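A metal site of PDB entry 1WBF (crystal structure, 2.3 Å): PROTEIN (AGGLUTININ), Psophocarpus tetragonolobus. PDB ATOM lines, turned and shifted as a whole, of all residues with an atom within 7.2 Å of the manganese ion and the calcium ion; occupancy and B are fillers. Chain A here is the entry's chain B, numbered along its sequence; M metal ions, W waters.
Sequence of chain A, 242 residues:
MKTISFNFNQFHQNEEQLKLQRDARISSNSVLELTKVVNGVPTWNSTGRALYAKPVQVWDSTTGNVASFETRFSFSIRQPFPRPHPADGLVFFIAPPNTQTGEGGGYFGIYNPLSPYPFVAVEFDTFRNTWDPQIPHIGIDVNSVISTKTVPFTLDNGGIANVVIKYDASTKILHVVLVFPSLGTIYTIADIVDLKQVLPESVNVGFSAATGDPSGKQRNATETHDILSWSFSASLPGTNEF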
ATOM      1  N   ASP A  88      15.974   8.041  37.429  1.00  0.00           N
ATOM      2  CA  ASP A  88      15.566   7.940  36.024  1.00  0.00           C
ATOM      3  C   ASP A  88      16.610   8.457  35.062  1.00  0.00           C
ATOM      4  O   ASP A  88      16.602   8.087  33.892  1.00  0.00           O
ATOM      5  CB  ASP A  88      14.269   8.707  35.774  1.00  0.00           C
ATOM      6  CG  ASP A  88      13.041   7.871  36.021  1.00  0.00           C
ATOM      7  OD1 ASP A  88      12.842   6.870  35.293  1.00  0.00           O
ATOM      8  OD2 ASP A  88      12.277   8.193  36.953  1.00  0.00           O
ATOM      9  N   GLY A  89      17.515   9.305  35.537  1.00  0.00           N
ATOM     10  CA  GLY A  89      18.534   9.832  34.664  1.00  0.00           C
ATOM     11  C   GLY A  89      18.690  11.330  34.796  1.00  0.00           C
ATOM     12  O   GLY A  89      18.041  11.943  35.627  1.00  0.00           O
ATOM     13  N   GLY A 105      10.243  11.697  36.942  1.00  0.00           N
ATOM     14  CA  GLY A 105      10.307  10.365  36.382  1.00  0.00           C
ATOM     15  C   GLY A 105      11.090  10.357  35.076  1.00  0.00           C
ATOM     16  O   GLY A 105      12.081  11.061  34.941  1.00  0.00           O
ATOM     17  N   GLY A 106      10.602   9.586  34.106  1.00  0.00           N
ATOM     18  CA  GLY A 106      11.262   9.501  32.809  1.00  0.00           C
ATOM     19  C   GLY A 106      11.172  10.743  31.930  1.00  0.00           C
ATOM     20  O   GLY A 106      11.501  10.685  30.763  1.00  0.00           O
ATOM     21  N   TYR A 107      10.671  11.843  32.503  1.00  0.00           N
ATOM     22  CA  TYR A 107      10.543  13.125  31.801  1.00  0.00           C
ATOM     23  C   TYR A 107      11.644  14.065  32.257  1.00  0.00           C
ATOM     24  O   TYR A 107      11.722  15.205  31.803  1.00  0.00           O
ATOM     25  CB  TYR A 107       9.167  13.754  32.055  1.00  0.00           C
ATOM     26  CG  TYR A 107       8.001  13.064  31.353  1.00  0.00           C
ATOM     27  CD1 TYR A 107       8.217  12.259  30.232  1.00  0.00           C
ATOM     28  CD2 TYR A 107       6.702  13.191  31.819  1.00  0.00           C
ATOM     29  CE1 TYR A 107       7.172  11.592  29.606  1.00  0.00           C
ATOM     30  CE2 TYR A 107       5.642  12.532  31.195  1.00  0.00           C
ATOM     31  CZ  TYR A 107       5.886  11.736  30.084  1.00  0.00           C
ATOM     32  OH  TYR A 107       4.875  11.034  29.471  1.00  0.00           O
ATOM     33  N   PHE A 108      12.454  13.605  33.224  1.00  0.00           N
ATOM     34  CA  PHE A 108      13.631  14.334  33.762  1.00  0.00           C
ATOM     35  C   PHE A 108      13.434  15.725  34.328  1.00  0.00           C
ATOM     36  O   PHE A 108      14.411  16.438  34.576  1.00  0.00           O
ATOM     37  CB  PHE A 108      14.724  14.407  32.689  1.00  0.00           C
ATOM     38  CG  PHE A 108      14.994  13.102  32.036  1.00  0.00           C
ATOM     39  CD1 PHE A 108      15.485  12.030  32.773  1.00  0.00           C
ATOM     40  CD2 PHE A 108      14.683  12.923  30.698  1.00  0.00           C
ATOM     41  CE1 PHE A 108      15.650  10.778  32.169  1.00  0.00           C
ATOM     42  CE2 PHE A 108      14.841  11.683  30.090  1.00  0.00           C
ATOM     43  CZ  PHE A 108      15.324  10.607  30.832  1.00  0.00           C
ATOM     44  N   GLU A 123      20.222  13.344  27.037  1.00  0.00           N
ATOM     45  CA  GLU A 123      19.921  12.607  28.245  1.00  0.00           C
ATOM     46  C   GLU A 123      20.922  11.493  28.434  1.00  0.00           C
ATOM     47  O   GLU A 123      21.602  11.105  27.500  1.00  0.00           O
ATOM     48  CB  GLU A 123      18.522  11.982  28.141  1.00  0.00           C
ATOM     49  CG  GLU A 123      18.368  11.275  26.839  1.00  0.00           C
ATOM     50  CD  GLU A 123      17.223  10.313  26.776  1.00  0.00           C
ATOM     51  OE1 GLU A 123      16.058  10.738  26.906  1.00  0.00           O
ATOM     52  OE2 GLU A 123      17.515   9.135  26.527  1.00  0.00           O
ATOM     53  N   PHE A 124      20.993  11.010  29.661  1.00  0.00           N
ATOM     54  CA  PHE A 124      21.826   9.899  30.070  1.00  0.00           C
ATOM     55  C   PHE A 124      20.738   9.208  30.850  1.00  0.00           C
ATOM     56  O   PHE A 124      20.350   9.622  31.943  1.00  0.00           O
ATOM     57  CB  PHE A 124      22.979  10.381  30.935  1.00  0.00           C
ATOM     58  CG  PHE A 124      23.872  11.363  30.221  1.00  0.00           C
ATOM     59  CD1 PHE A 124      24.893  10.922  29.390  1.00  0.00           C
ATOM     60  CD2 PHE A 124      23.638  12.732  30.307  1.00  0.00           C
ATOM     61  CE1 PHE A 124      25.669  11.840  28.661  1.00  0.00           C
ATOM     62  CE2 PHE A 124      24.406  13.646  29.582  1.00  0.00           C
ATOM     63  CZ  PHE A 124      25.420  13.193  28.751  1.00  0.00           C
ATOM     64  N   ASP A 125      20.136   8.249  30.180  1.00  0.00           N
ATOM     65  CA  ASP A 125      18.988   7.552  30.687  1.00  0.00           C
ATOM     66  C   ASP A 125      19.300   6.238  31.342  1.00  0.00           C
ATOM     67  O   ASP A 125      19.815   5.324  30.716  1.00  0.00           O
ATOM     68  CB  ASP A 125      18.019   7.342  29.530  1.00  0.00           C
ATOM     69  CG  ASP A 125      16.590   7.136  29.974  1.00  0.00           C
ATOM     70  OD1 ASP A 125      16.353   6.365  30.908  1.00  0.00           O
ATOM     71  OD2 ASP A 125      15.696   7.749  29.396  1.00  0.00           O
ATOM     72  N   THR A 126      18.755   6.085  32.536  1.00  0.00           N
ATOM     73  CA  THR A 126      18.973   4.891  33.310  1.00  0.00           C
ATOM     74  C   THR A 126      17.772   3.982  33.508  1.00  0.00           C
ATOM     75  O   THR A 126      17.912   2.849  33.959  1.00  0.00           O
ATOM     76  CB  THR A 126      19.562   5.271  34.678  1.00  0.00           C
ATOM     77  OG1 THR A 126      18.633   6.137  35.362  1.00  0.00           O
ATOM     78  CG2 THR A 126      20.866   6.042  34.492  1.00  0.00           C
ATOM     79  N   PHE A 127      16.581   4.443  33.133  1.00  0.00           N
ATOM     80  CA  PHE A 127      15.382   3.637  33.305  1.00  0.00           C
ATOM     81  C   PHE A 127      14.679   3.370  31.950  1.00  0.00           C
ATOM     82  O   PHE A 127      14.446   4.280  31.177  1.00  0.00           O
ATOM     83  CB  PHE A 127      14.439   4.298  34.324  1.00  0.00           C
ATOM     84  CG  PHE A 127      13.251   3.466  34.662  1.00  0.00           C
ATOM     85  CD1 PHE A 127      13.383   2.337  35.462  1.00  0.00           C
ATOM     86  CD2 PHE A 127      12.014   3.754  34.106  1.00  0.00           C
ATOM     87  CE1 PHE A 127      12.299   1.501  35.680  1.00  0.00           C
ATOM     88  CE2 PHE A 127      10.922   2.913  34.328  1.00  0.00           C
ATOM     89  CZ  PHE A 127      11.070   1.792  35.119  1.00  0.00           C
ATOM     90  N   ARG A 128      14.379   2.111  31.642  1.00  0.00           N
ATOM     91  CA  ARG A 128      13.748   1.805  30.362  1.00  0.00           C
ATOM     92  C   ARG A 128      12.225   1.925  30.311  1.00  0.00           C
ATOM     93  O   ARG A 128      11.506   0.956  30.594  1.00  0.00           O
ATOM     94  CB  ARG A 128      14.176   0.431  29.865  1.00  0.00           C
ATOM     95  CG  ARG A 128      13.781   0.183  28.418  1.00  0.00           C
ATOM     96  CD  ARG A 128      14.159  -1.202  27.954  1.00  0.00           C
ATOM     97  NE  ARG A 128      13.734  -1.432  26.575  1.00  0.00           N
ATOM     98  CZ  ARG A 128      14.101  -2.468  25.840  1.00  0.00           C
ATOM     99  NH1 ARG A 128      14.906  -3.399  26.331  1.00  0.00           N
ATOM    100  NH2 ARG A 128      13.652  -2.592  24.602  1.00  0.00           N
ATOM    101  N   ASN A 129      11.732   3.104  29.922  1.00  0.00           N
ATOM    102  CA  ASN A 129      10.296   3.351  29.776  1.00  0.00           C
ATOM    103  C   ASN A 129       9.793   2.616  28.529  1.00  0.00           C
ATOM    104  O   ASN A 129      10.572   2.022  27.806  1.00  0.00           O
ATOM    105  CB  ASN A 129      10.032   4.844  29.605  1.00  0.00           C
ATOM    106  CG  ASN A 129      10.265   5.618  30.861  1.00  0.00           C
ATOM    107  OD1 ASN A 129      11.377   6.060  31.121  1.00  0.00           O
ATOM    108  ND2 ASN A 129       9.207   5.867  31.616  1.00  0.00           N
ATOM    109  N   THR A 130       8.500   2.706  28.239  1.00  0.00           N
ATOM    110  CA  THR A 130       7.962   2.016  27.050  1.00  0.00           C
ATOM    111  C   THR A 130       8.483   2.577  25.711  1.00  0.00           C
ATOM    112  O   THR A 130       8.552   1.866  24.700  1.00  0.00           O
ATOM    113  CB  THR A 130       6.403   2.043  27.041  1.00  0.00           C
ATOM    114  OG1 THR A 130       5.950   3.355  27.386  1.00  0.00           O
ATOM    115  CG2 THR A 130       5.850   1.022  28.033  1.00  0.00           C
ATOM    116  N   TRP A 131       8.826   3.853  25.704  1.00  0.00           N
ATOM    117  CA  TRP A 131       9.327   4.526  24.517  1.00  0.00           C
ATOM    118  C   TRP A 131      10.844   4.439  24.389  1.00  0.00           C
ATOM    119  O   TRP A 131      11.432   4.962  23.432  1.00  0.00           O
ATOM    120  CB  TRP A 131       8.946   5.978  24.601  1.00  0.00           C
ATOM    121  CG  TRP A 131       9.527   6.635  25.798  1.00  0.00           C
ATOM    122  CD1 TRP A 131      10.797   7.107  25.950  1.00  0.00           C
ATOM    123  CD2 TRP A 131       8.823   6.979  26.995  1.00  0.00           C
ATOM    124  NE1 TRP A 131      10.916   7.749  27.147  1.00  0.00           N
ATOM    125  CE2 TRP A 131       9.717   7.694  27.820  1.00  0.00           C
ATOM    126  CE3 TRP A 131       7.520   6.767  27.460  1.00  0.00           C
ATOM    127  CZ2 TRP A 131       9.359   8.201  29.073  1.00  0.00           C
ATOM    128  CZ3 TRP A 131       7.155   7.277  28.705  1.00  0.00           C
ATOM    129  CH2 TRP A 131       8.072   7.979  29.495  1.00  0.00           C
ATOM    130  N   ASP A 132      11.491   3.852  25.388  1.00  0.00           N
ATOM    131  CA  ASP A 132      12.945   3.715  25.433  1.00  0.00           C
ATOM    132  C   ASP A 132      13.476   2.380  24.953  1.00  0.00           C
ATOM    133  O   ASP A 132      12.784   1.384  25.008  1.00  0.00           O
ATOM    134  CB  ASP A 132      13.425   3.833  26.869  1.00  0.00           C
ATOM    135  CG  ASP A 132      13.643   5.222  27.279  1.00  0.00           C
ATOM    136  OD1 ASP A 132      14.207   5.990  26.479  1.00  0.00           O
ATOM    137  OD2 ASP A 132      13.231   5.529  28.399  1.00  0.00           O
ATOM    138  N   PRO A 133      14.727   2.369  24.425  1.00  0.00           N
ATOM    139  CA  PRO A 133      15.426   1.176  23.954  1.00  0.00           C
ATOM    140  C   PRO A 133      16.322   0.778  25.157  1.00  0.00           C
ATOM    141  O   PRO A 133      16.437   1.564  26.112  1.00  0.00           O
ATOM    142  CB  PRO A 133      16.270   1.729  22.802  1.00  0.00           C
ATOM    143  CG  PRO A 133      16.682   3.051  23.328  1.00  0.00           C
ATOM    144  CD  PRO A 133      15.375   3.591  23.888  1.00  0.00           C
ATOM    145  N   ILE A 135      18.675   0.121  28.263  1.00  0.00           N
ATOM    146  CA  ILE A 135      19.358   1.110  29.095  1.00  0.00           C
ATOM    147  C   ILE A 135      20.669   0.579  29.707  1.00  0.00           C
ATOM    148  O   ILE A 135      20.866  -0.634  29.818  1.00  0.00           O
ATOM    149  CB  ILE A 135      18.443   1.629  30.247  1.00  0.00           C
ATOM    150  CG1 ILE A 135      17.679   0.475  30.910  1.00  0.00           C
ATOM    151  CG2 ILE A 135      17.502   2.676  29.734  1.00  0.00           C
ATOM    152  CD1 ILE A 135      18.519  -0.408  31.854  1.00  0.00           C
ATOM    153  N   HIS A 137      21.544   4.523  28.071  1.00  0.00           N
ATOM    154  CA  HIS A 137      21.894   4.994  26.733  1.00  0.00           C
ATOM    155  C   HIS A 137      21.932   6.492  26.743  1.00  0.00           C
ATOM    156  O   HIS A 137      21.321   7.116  27.629  1.00  0.00           O
ATOM    157  CB  HIS A 137      20.896   4.509  25.645  1.00  0.00           C
ATOM    158  CG  HIS A 137      19.457   4.881  25.921  1.00  0.00           C
ATOM    159  ND1 HIS A 137      18.476   3.937  26.110  1.00  0.00           N
ATOM    160  CD2 HIS A 137      18.850   6.072  26.084  1.00  0.00           C
ATOM    161  CE1 HIS A 137      17.338   4.521  26.402  1.00  0.00           C
ATOM    162  NE2 HIS A 137      17.537   5.838  26.389  1.00  0.00           N
ATOM    163  N   ILE A 138      22.749   7.066  25.857  1.00  0.00           N
ATOM    164  CA  ILE A 138      22.807   8.524  25.705  1.00  0.00           C
ATOM    165  C   ILE A 138      21.733   8.782  24.645  1.00  0.00           C
ATOM    166  O   ILE A 138      21.513   7.928  23.755  1.00  0.00           O
ATOM    167  CB  ILE A 138      24.125   9.008  25.062  1.00  0.00           C
ATOM    168  CG1 ILE A 138      25.343   8.517  25.840  1.00  0.00           C
ATOM    169  CG2 ILE A 138      24.131  10.545  24.942  1.00  0.00           C
ATOM    170  CD1 ILE A 138      26.652   8.768  25.097  1.00  0.00           C
ATOM    171  N   GLY A 139      21.104   9.950  24.670  1.00  0.00           N
ATOM    172  CA  GLY A 139      20.089  10.216  23.675  1.00  0.00           C
ATOM    173  C   GLY A 139      19.897  11.674  23.369  1.00  0.00           C
ATOM    174  O   GLY A 139      20.062  12.518  24.244  1.00  0.00           O
ATOM    175  N   ASP A 141      17.383  14.590  22.365  1.00  0.00           N
ATOM    176  CA  ASP A 141      15.966  14.880  22.473  1.00  0.00           C
ATOM    177  C   ASP A 141      15.578  16.214  21.869  1.00  0.00           C
ATOM    178  O   ASP A 141      16.127  17.245  22.226  1.00  0.00           O
ATOM    179  CB  ASP A 141      15.564  14.913  23.962  1.00  0.00           C
ATOM    180  CG  ASP A 141      15.759  13.585  24.661  1.00  0.00           C
ATOM    181  OD1 ASP A 141      15.920  12.528  23.980  1.00  0.00           O
ATOM    182  OD2 ASP A 141      15.718  13.595  25.907  1.00  0.00           O
ATOM    183  N   VAL A 145      10.748  13.316  24.861  1.00  0.00           N
ATOM    184  CA  VAL A 145      11.650  12.308  25.419  1.00  0.00           C
ATOM    185  C   VAL A 145      11.783  11.044  24.584  1.00  0.00           C
ATOM    186  O   VAL A 145      12.214  10.016  25.081  1.00  0.00           O
ATOM    187  CB  VAL A 145      11.358  11.921  26.919  1.00  0.00           C
ATOM    188  CG1 VAL A 145      11.643  13.097  27.837  1.00  0.00           C
ATOM    189  CG2 VAL A 145       9.929  11.416  27.084  1.00  0.00           C
ATOM    190  N   ILE A 146      11.332  11.108  23.330  1.00  0.00           N
ATOM    191  CA  ILE A 146      11.485   9.961  22.423  1.00  0.00           C
ATOM    192  C   ILE A 146      12.635  10.438  21.549  1.00  0.00           C
ATOM    193  O   ILE A 146      12.444  11.174  20.595  1.00  0.00           O
ATOM    194  CB  ILE A 146      10.228   9.685  21.548  1.00  0.00           C
ATOM    195  CG1 ILE A 146       8.989   9.519  22.431  1.00  0.00           C
ATOM    196  CG2 ILE A 146      10.415   8.384  20.777  1.00  0.00           C
ATOM    197  CD1 ILE A 146       7.763   9.016  21.679  1.00  0.00           C
ATOM    198  N   SER A 147      13.835  10.045  21.945  1.00  0.00           N
ATOM    199  CA  SER A 147      15.049  10.448  21.256  1.00  0.00           C
ATOM    200  C   SER A 147      15.092  10.220  19.749  1.00  0.00           C
ATOM    201  O   SER A 147      14.630   9.194  19.249  1.00  0.00           O
ATOM    202  CB  SER A 147      16.265   9.785  21.926  1.00  0.00           C
ATOM    203  OG  SER A 147      16.215   9.935  23.342  1.00  0.00           O
ATOM    204  N   THR A 150      19.962   7.440  19.502  1.00  0.00           N
ATOM    205  CA  THR A 150      20.497   6.931  20.788  1.00  0.00           C
ATOM    206  C   THR A 150      21.680   5.976  20.641  1.00  0.00           C
ATOM    207  O   THR A 150      21.904   5.411  19.559  1.00  0.00           O
ATOM    208  CB  THR A 150      19.443   6.173  21.621  1.00  0.00           C
ATOM    209  OG1 THR A 150      19.090   4.969  20.966  1.00  0.00           O
ATOM    210  CG2 THR A 150      18.206   7.006  21.839  1.00  0.00           C
HETATM  211 MN    MN M   1      15.718   7.735  26.806  1.00  0.00          MN
HETATM  212 CA    CA M   2      13.684   6.329  30.579  1.00  0.00          CA
HETATM  213  O   HOH W   1      12.970   8.930  29.681  1.00  0.00           O
HETATM  214  O   HOH W   2      15.614   7.302  24.457  1.00  0.00           O
HETATM  215  O   HOH W   3      14.064   9.129  27.012  1.00  0.00           O
HETATM  216  O   HOH W   4      13.937   7.292  32.765  1.00  0.00           O
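Of the 26 residues printed, 4 come within 4 Å of the calcium ion.
Water W3 is bound to the manganese ion, at 2.2 Å. The manganese ion is bound by the side-chain carboxylate (OE2) of Glu 123. The manganese ion is bound by OD1 of Asp 132, 2.3 Å away. Water W2 is bound to the manganese ion (2.4 Å). OD2 of Asp 125 is bound to the manganese ion, at 2.6 Å. The manganese ion is bound by NE2 of His 137, at 2.7 Å.
Water W3 lies within hydrogen-bond range of OE1 of Glu 123, O of Val 145 and NE1 of Trp 131. Water W1 bridges the backbone carbonyl oxygen (O) of Gly 106 and the indole nitrogen (NE1) of Trp 131.
The backbone carbonyl oxygen of Gly 139 sits at hydrogen-bond distance from the backbone NH of Glu 123 (2.9 Å). NE1 of Trp 131 lies close to OD2 of Asp 132, 3.4 Å away. A ring nitrogen (ND1) of His 137 sits close to the backbone carbonyl oxygen (O) of Pro 133 (3.1 Å). The backbone carbonyl oxygen (O) of Asp 132 is in hydrogen-bond range of the guanidinium group (NE) of Arg 128.
O of Phe 127 is bound to the calcium ion, at 2.3 Å. OD2 of Asp 132 is bound to the calcium ion. OD1 of Asn 129 binds the calcium ion, at 2.4 Å. Water W4 binds the calcium ion, at 2.4 Å. The calcium ion is bound by OD1 of Asp 125, 2.7 Å away. OD2 of Asp 125 is bound to the calcium ion (2.7 Å). The calcium ion is bound by water W1. The calcium ion has seven donor atoms within binding distance.
Of the 26 residues printed, 4 come within 4 Å of the manganese ion. The nearest printed residue that does not touch the manganese ion is Ser 147 (4.1 Å).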
